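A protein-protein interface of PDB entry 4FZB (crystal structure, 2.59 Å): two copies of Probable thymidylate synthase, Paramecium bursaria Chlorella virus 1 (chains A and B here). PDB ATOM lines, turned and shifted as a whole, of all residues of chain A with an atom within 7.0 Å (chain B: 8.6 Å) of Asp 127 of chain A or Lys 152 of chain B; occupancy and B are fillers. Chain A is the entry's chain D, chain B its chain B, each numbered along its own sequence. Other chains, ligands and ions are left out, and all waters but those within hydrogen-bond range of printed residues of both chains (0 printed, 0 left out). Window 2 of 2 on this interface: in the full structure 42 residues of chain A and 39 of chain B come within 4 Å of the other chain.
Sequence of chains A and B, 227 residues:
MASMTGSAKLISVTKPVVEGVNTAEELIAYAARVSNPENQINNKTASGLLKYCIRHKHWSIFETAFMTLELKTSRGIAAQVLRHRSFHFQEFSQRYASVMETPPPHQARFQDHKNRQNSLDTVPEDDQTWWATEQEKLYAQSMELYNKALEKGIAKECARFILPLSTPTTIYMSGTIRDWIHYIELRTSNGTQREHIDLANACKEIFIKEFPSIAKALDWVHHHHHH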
ATOM      1  N   ALA A 108     -16.820  29.239  10.247  1.00  0.00           N
ATOM      2  CA  ALA A 108     -16.254  28.687  11.478  1.00  0.00           C
ATOM      3  C   ALA A 108     -14.721  28.816  11.514  1.00  0.00           C
ATOM      4  O   ALA A 108     -14.065  28.947  10.475  1.00  0.00           O
ATOM      5  CB  ALA A 108     -16.644  27.226  11.620  1.00  0.00           C
ATOM      6  N   PHE A 110     -11.279  27.718  14.656  1.00  0.00           N
ATOM      7  CA  PHE A 110     -10.955  26.851  15.788  1.00  0.00           C
ATOM      8  C   PHE A 110     -10.455  27.613  17.007  1.00  0.00           C
ATOM      9  O   PHE A 110     -10.643  27.156  18.131  1.00  0.00           O
ATOM     10  CB  PHE A 110      -9.956  25.765  15.347  1.00  0.00           C
ATOM     11  CG  PHE A 110     -10.545  24.586  14.598  1.00  0.00           C
ATOM     12  CD1 PHE A 110      -9.956  23.331  14.676  1.00  0.00           C
ATOM     13  CD2 PHE A 110     -11.700  24.726  13.829  1.00  0.00           C
ATOM     14  CE1 PHE A 110     -10.504  22.242  13.998  1.00  0.00           C
ATOM     15  CE2 PHE A 110     -12.248  23.636  13.155  1.00  0.00           C
ATOM     16  CZ  PHE A 110     -11.642  22.402  13.238  1.00  0.00           C
ATOM     17  N   GLU A 125     -11.985  22.614   4.667  1.00  0.00           N
ATOM     18  CA  GLU A 125     -12.927  22.846   3.571  1.00  0.00           C
ATOM     19  C   GLU A 125     -14.119  21.882   3.687  1.00  0.00           C
ATOM     20  O   GLU A 125     -15.261  22.282   3.424  1.00  0.00           O
ATOM     21  CB  GLU A 125     -12.229  22.704   2.196  1.00  0.00           C
ATOM     22  CG  GLU A 125     -13.088  23.079   0.984  1.00  0.00           C
ATOM     23  CD  GLU A 125     -13.284  22.016  -0.089  1.00  0.00           C
ATOM     24  OE1 GLU A 125     -14.094  21.083   0.124  1.00  0.00           O
ATOM     25  OE2 GLU A 125     -12.674  22.153  -1.174  1.00  0.00           O
ATOM     26  N   ASP A 126     -13.839  20.611   4.053  1.00  0.00           N
ATOM     27  CA  ASP A 126     -14.856  19.570   4.198  1.00  0.00           C
ATOM     28  C   ASP A 126     -15.595  19.739   5.502  1.00  0.00           C
ATOM     29  O   ASP A 126     -16.812  19.538   5.533  1.00  0.00           O
ATOM     30  CB  ASP A 126     -14.270  18.160   4.016  1.00  0.00           C
ATOM     31  CG  ASP A 126     -13.909  17.823   2.575  1.00  0.00           C
ATOM     32  OD1 ASP A 126     -14.656  18.250   1.653  1.00  0.00           O
ATOM     33  OD2 ASP A 126     -12.882  17.132   2.362  1.00  0.00           O
ATOM     34  N   ASP A 127     -14.872  20.182   6.559  1.00  0.00           N
ATOM     35  CA  ASP A 127     -15.453  20.489   7.867  1.00  0.00           C
ATOM     36  C   ASP A 127     -16.215  21.815   7.772  1.00  0.00           C
ATOM     37  O   ASP A 127     -17.298  21.951   8.334  1.00  0.00           O
ATOM     38  CB  ASP A 127     -14.367  20.544   8.951  1.00  0.00           C
ATOM     39  CG  ASP A 127     -13.650  19.217   9.171  1.00  0.00           C
ATOM     40  OD1 ASP A 127     -12.406  19.179   9.007  1.00  0.00           O
ATOM     41  OD2 ASP A 127     -14.333  18.216   9.518  1.00  0.00           O
ATOM     42  N   GLN A 128     -15.658  22.771   7.011  1.00  0.00           N
ATOM     43  CA  GLN A 128     -16.263  24.062   6.726  1.00  0.00           C
ATOM     44  C   GLN A 128     -17.578  23.851   5.936  1.00  0.00           C
ATOM     45  O   GLN A 128     -18.611  24.422   6.296  1.00  0.00           O
ATOM     46  CB  GLN A 128     -15.266  24.961   5.971  1.00  0.00           C
ATOM     47  CG  GLN A 128     -15.644  26.452   5.916  1.00  0.00           C
ATOM     48  CD  GLN A 128     -15.815  27.119   7.269  1.00  0.00           C
ATOM     49  OE1 GLN A 128     -14.831  27.505   7.924  1.00  0.00           O
ATOM     50  NE2 GLN A 128     -17.079  27.291   7.698  1.00  0.00           N
ATOM     51  N   THR A 129     -17.557  22.976   4.916  1.00  0.00           N
ATOM     52  CA  THR A 129     -18.754  22.649   4.140  1.00  0.00           C
ATOM     53  C   THR A 129     -19.874  22.116   5.047  1.00  0.00           C
ATOM     54  O   THR A 129     -20.993  22.628   4.982  1.00  0.00           O
ATOM     55  CB  THR A 129     -18.396  21.768   2.936  1.00  0.00           C
ATOM     56  OG1 THR A 129     -17.747  22.596   1.961  1.00  0.00           O
ATOM     57  CG2 THR A 129     -19.614  21.073   2.319  1.00  0.00           C
ATOM     58  N   TRP A 130     -19.542  21.138   5.926  1.00  0.00           N
ATOM     59  CA  TRP A 130     -20.461  20.517   6.884  1.00  0.00           C
ATOM     60  C   TRP A 130     -21.193  21.596   7.664  1.00  0.00           C
ATOM     61  O   TRP A 130     -22.423  21.582   7.713  1.00  0.00           O
ATOM     62  CB  TRP A 130     -19.705  19.564   7.848  1.00  0.00           C
ATOM     63  CG  TRP A 130     -20.508  19.127   9.052  1.00  0.00           C
ATOM     64  CD1 TRP A 130     -21.403  18.098   9.115  1.00  0.00           C
ATOM     65  CD2 TRP A 130     -20.521  19.752  10.345  1.00  0.00           C
ATOM     66  NE1 TRP A 130     -21.940  18.012  10.383  1.00  0.00           N
ATOM     67  CE2 TRP A 130     -21.436  19.032  11.149  1.00  0.00           C
ATOM     68  CE3 TRP A 130     -19.863  20.862  10.899  1.00  0.00           C
ATOM     69  CZ2 TRP A 130     -21.668  19.361  12.485  1.00  0.00           C
ATOM     70  CZ3 TRP A 130     -20.124  21.204  12.212  1.00  0.00           C
ATOM     71  CH2 TRP A 130     -20.995  20.445  13.000  1.00  0.00           C
ATOM     72  N   TRP A 131     -20.426  22.547   8.235  1.00  0.00           N
ATOM     73  CA  TRP A 131     -20.916  23.672   9.012  1.00  0.00           C
ATOM     74  C   TRP A 131     -21.867  24.576   8.241  1.00  0.00           C
ATOM     75  O   TRP A 131     -22.897  24.949   8.789  1.00  0.00           O
ATOM     76  CB  TRP A 131     -19.737  24.460   9.573  1.00  0.00           C
ATOM     77  CG  TRP A 131     -20.113  25.587  10.489  1.00  0.00           C
ATOM     78  CD1 TRP A 131     -19.779  26.899  10.338  1.00  0.00           C
ATOM     79  CD2 TRP A 131     -20.852  25.496  11.714  1.00  0.00           C
ATOM     80  NE1 TRP A 131     -20.252  27.633  11.395  1.00  0.00           N
ATOM     81  CE2 TRP A 131     -20.919  26.798  12.258  1.00  0.00           C
ATOM     82  CE3 TRP A 131     -21.520  24.449  12.383  1.00  0.00           C
ATOM     83  CZ2 TRP A 131     -21.607  27.078  13.451  1.00  0.00           C
ATOM     84  CZ3 TRP A 131     -22.204  24.736  13.558  1.00  0.00           C
ATOM     85  CH2 TRP A 131     -22.231  26.032  14.083  1.00  0.00           C
ATOM     86  N   ALA A 132     -21.539  24.921   6.982  1.00  0.00           N
ATOM     87  CA  ALA A 132     -22.391  25.787   6.156  1.00  0.00           C
ATOM     88  C   ALA A 132     -23.727  25.104   5.829  1.00  0.00           C
ATOM     89  O   ALA A 132     -24.779  25.716   6.013  1.00  0.00           O
ATOM     90  CB  ALA A 132     -21.667  26.182   4.875  1.00  0.00           C
ATOM     91  N   LEU B 145     -26.533  20.205  16.786  1.00  0.00           N
ATOM     92  CA  LEU B 145     -25.581  20.892  15.917  1.00  0.00           C
ATOM     93  C   LEU B 145     -24.518  21.702  16.726  1.00  0.00           C
ATOM     94  O   LEU B 145     -23.339  21.683  16.354  1.00  0.00           O
ATOM     95  CB  LEU B 145     -26.302  21.723  14.822  1.00  0.00           C
ATOM     96  CG  LEU B 145     -25.431  22.557  13.842  1.00  0.00           C
ATOM     97  CD1 LEU B 145     -24.341  21.743  13.191  1.00  0.00           C
ATOM     98  CD2 LEU B 145     -26.267  23.249  12.798  1.00  0.00           C
ATOM     99  N   TYR B 146     -24.933  22.345  17.852  1.00  0.00           N
ATOM    100  CA  TYR B 146     -24.059  23.130  18.730  1.00  0.00           C
ATOM    101  C   TYR B 146     -23.014  22.226  19.317  1.00  0.00           C
ATOM    102  O   TYR B 146     -21.840  22.429  19.044  1.00  0.00           O
ATOM    103  CB  TYR B 146     -24.860  23.868  19.832  1.00  0.00           C
ATOM    104  CG  TYR B 146     -24.009  24.702  20.769  1.00  0.00           C
ATOM    105  CD1 TYR B 146     -23.549  24.182  21.971  1.00  0.00           C
ATOM    106  CD2 TYR B 146     -23.653  26.008  20.446  1.00  0.00           C
ATOM    107  CE1 TYR B 146     -22.744  24.934  22.824  1.00  0.00           C
ATOM    108  CE2 TYR B 146     -22.851  26.773  21.289  1.00  0.00           C
ATOM    109  CZ  TYR B 146     -22.393  26.230  22.477  1.00  0.00           C
ATOM    110  OH  TYR B 146     -21.611  26.968  23.334  1.00  0.00           O
ATOM    111  N   ASN B 147     -23.437  21.199  20.067  1.00  0.00           N
ATOM    112  CA  ASN B 147     -22.557  20.205  20.681  1.00  0.00           C
ATOM    113  C   ASN B 147     -21.628  19.549  19.641  1.00  0.00           C
ATOM    114  O   ASN B 147     -20.441  19.392  19.930  1.00  0.00           O
ATOM    115  CB  ASN B 147     -23.364  19.149  21.489  1.00  0.00           C
ATOM    116  CG  ASN B 147     -24.223  19.696  22.635  1.00  0.00           C
ATOM    117  OD1 ASN B 147     -23.774  20.424  23.526  1.00  0.00           O
ATOM    118  ND2 ASN B 147     -25.479  19.303  22.674  1.00  0.00           N
ATOM    119  N   LYS B 148     -22.133  19.242  18.418  1.00  0.00           N
ATOM    120  CA  LYS B 148     -21.286  18.651  17.372  1.00  0.00           C
ATOM    121  C   LYS B 148     -20.170  19.594  16.966  1.00  0.00           C
ATOM    122  O   LYS B 148     -19.029  19.147  16.846  1.00  0.00           O
ATOM    123  CB  LYS B 148     -22.079  18.180  16.140  1.00  0.00           C
ATOM    124  CG  LYS B 148     -22.858  16.897  16.369  1.00  0.00           C
ATOM    125  CD  LYS B 148     -22.373  15.733  15.510  1.00  0.00           C
ATOM    126  CE  LYS B 148     -23.347  14.569  15.547  1.00  0.00           C
ATOM    127  NZ  LYS B 148     -24.623  14.856  14.819  1.00  0.00           N
ATOM    128  N   ALA B 149     -20.490  20.898  16.785  1.00  0.00           N
ATOM    129  CA  ALA B 149     -19.540  21.954  16.407  1.00  0.00           C
ATOM    130  C   ALA B 149     -18.382  22.059  17.408  1.00  0.00           C
ATOM    131  O   ALA B 149     -17.228  22.096  16.993  1.00  0.00           O
ATOM    132  CB  ALA B 149     -20.256  23.289  16.264  1.00  0.00           C
ATOM    133  N   LEU B 150     -18.689  22.018  18.720  1.00  0.00           N
ATOM    134  CA  LEU B 150     -17.678  22.041  19.788  1.00  0.00           C
ATOM    135  C   LEU B 150     -16.930  20.727  19.869  1.00  0.00           C
ATOM    136  O   LEU B 150     -15.733  20.731  20.164  1.00  0.00           O
ATOM    137  CB  LEU B 150     -18.286  22.369  21.153  1.00  0.00           C
ATOM    138  CG  LEU B 150     -19.082  23.644  21.288  1.00  0.00           C
ATOM    139  CD1 LEU B 150     -19.346  23.895  22.725  1.00  0.00           C
ATOM    140  CD2 LEU B 150     -18.351  24.843  20.664  1.00  0.00           C
ATOM    141  N   GLU B 151     -17.617  19.604  19.605  1.00  0.00           N
ATOM    142  CA  GLU B 151     -16.942  18.312  19.534  1.00  0.00           C
ATOM    143  C   GLU B 151     -15.908  18.421  18.394  1.00  0.00           C
ATOM    144  O   GLU B 151     -14.748  18.088  18.613  1.00  0.00           O
ATOM    145  CB  GLU B 151     -17.934  17.159  19.270  1.00  0.00           C
ATOM    146  CG  GLU B 151     -18.620  16.627  20.527  1.00  0.00           C
ATOM    147  CD  GLU B 151     -19.905  15.824  20.351  1.00  0.00           C
ATOM    148  OE1 GLU B 151     -20.143  15.295  19.240  1.00  0.00           O
ATOM    149  OE2 GLU B 151     -20.667  15.705  21.342  1.00  0.00           O
ATOM    150  N   LYS B 152     -16.309  19.019  17.234  1.00  0.00           N
ATOM    151  CA  LYS B 152     -15.478  19.221  16.035  1.00  0.00           C
ATOM    152  C   LYS B 152     -14.358  20.265  16.203  1.00  0.00           C
ATOM    153  O   LYS B 152     -13.556  20.466  15.277  1.00  0.00           O
ATOM    154  CB  LYS B 152     -16.343  19.551  14.801  1.00  0.00           C
ATOM    155  CG  LYS B 152     -17.057  18.335  14.214  1.00  0.00           C
ATOM    156  CD  LYS B 152     -17.758  18.610  12.887  1.00  0.00           C
ATOM    157  CE  LYS B 152     -16.835  18.647  11.684  1.00  0.00           C
ATOM    158  NZ  LYS B 152     -16.262  17.307  11.367  1.00  0.00           N
ATOM    159  N   GLY B 153     -14.332  20.920  17.362  1.00  0.00           N
ATOM    160  CA  GLY B 153     -13.344  21.935  17.700  1.00  0.00           C
ATOM    161  C   GLY B 153     -13.612  23.334  17.174  1.00  0.00           C
ATOM    162  O   GLY B 153     -12.690  24.161  17.163  1.00  0.00           O
ATOM    163  N   ILE B 154     -14.865  23.630  16.736  1.00  0.00           N
ATOM    164  CA  ILE B 154     -15.224  24.972  16.239  1.00  0.00           C
ATOM    165  C   ILE B 154     -15.189  25.936  17.420  1.00  0.00           C
ATOM    166  O   ILE B 154     -15.450  25.503  18.545  1.00  0.00           O
ATOM    167  CB  ILE B 154     -16.551  24.995  15.408  1.00  0.00           C
ATOM    168  CG1 ILE B 154     -16.328  24.309  14.038  1.00  0.00           C
ATOM    169  CG2 ILE B 154     -17.095  26.405  15.198  1.00  0.00           C
ATOM    170  CD1 ILE B 154     -17.513  23.488  13.494  1.00  0.00           C
ATOM    171  N   ALA B 155     -14.750  27.197  17.189  1.00  0.00           N
ATOM    172  CA  ALA B 155     -14.672  28.228  18.231  1.00  0.00           C
ATOM    173  C   ALA B 155     -16.089  28.559  18.750  1.00  0.00           C
ATOM    174  O   ALA B 155     -17.030  28.575  17.957  1.00  0.00           O
ATOM    175  CB  ALA B 155     -13.990  29.468  17.682  1.00  0.00           C
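NZ of Lys 152 of chain B lies within salt-bridge range of OD2 of Asp 127 of chain A (2.8 Å).
O of Ala 108 of chain A sits close to OE1 of Gln 128 of chain A.
O of Ala 149 of chain B sits at hydrogen-bond distance from N of Ile 154 of chain B, 2.8 Å away.
Among the printed residues, merely in contact across the chains: Phe 110 of chain A with Gly 153 of chain B, Phe 110 of chain A with Lys 152 of chain B, Trp 130 of chain A with Lys 152 of chain B, Trp 130 of chain A with Leu 145 of chain B, Trp 131 of chain A with Ala 149 of chain B, Trp 131 of chain A with Leu 145 of chain B, Trp 130 of chain A with Ile 154 of chain B, Ala 108 of chain A with Ile 154 of chain B, Trp 130 of chain A with Ala 149 of chain B and Trp 130 of chain A with Lys 148 of chain B.
Of chain A, only Phe 110, Asp 127 and Trp 130 come within 4 Å of Lys 152 of chain B.
Printed residues of chain B within 4 Å of Trp 131 of chain A: Leu 145 (3.7 Å) and Ala 149 (3.6 Å).
Printed residues of chain B within 4 Å of Ala 108 of chain A: Ile 154.
Printed residues of chain A within 4 Å of Gly 153 of chain B: Phe 110.
Of the printed residues of chain A, Ile 154 of chain B touches Ala 108 and Trp 130.
Of the printed residues of chain B, Trp 130 of chain A touches Leu 145, Lys 148, Ala 149, Lys 152 and Ile 154.
Asn 147 of chain B touches none of the printed residues of chain A.
Thr 129 of chain A touches none of the printed residues of chain B.
The nearest residue of chain A that does not touch Lys 152 of chain B is Asp 126 of chain A (6.2 Å).
The nearest printed residue of chain B that does not touch Ala 108 of chain A is Ala 155 of chain B (5.9 Å).
Of the 11 printed residues of chain B, 6 touch a printed residue of chain A.
Hydrophobic or aromatic side chains of chain B within 4 Å of the printed part of chain A: Leu 145, Ala 149 and Ile 154.
Of the 10 printed residues of chain A, 5 touch a printed residue of chain B.
No position is printed for both chains.
Of the 11 pairs that touch across the chains among the printed residues, none has its exchanged pair printed and touching as well.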
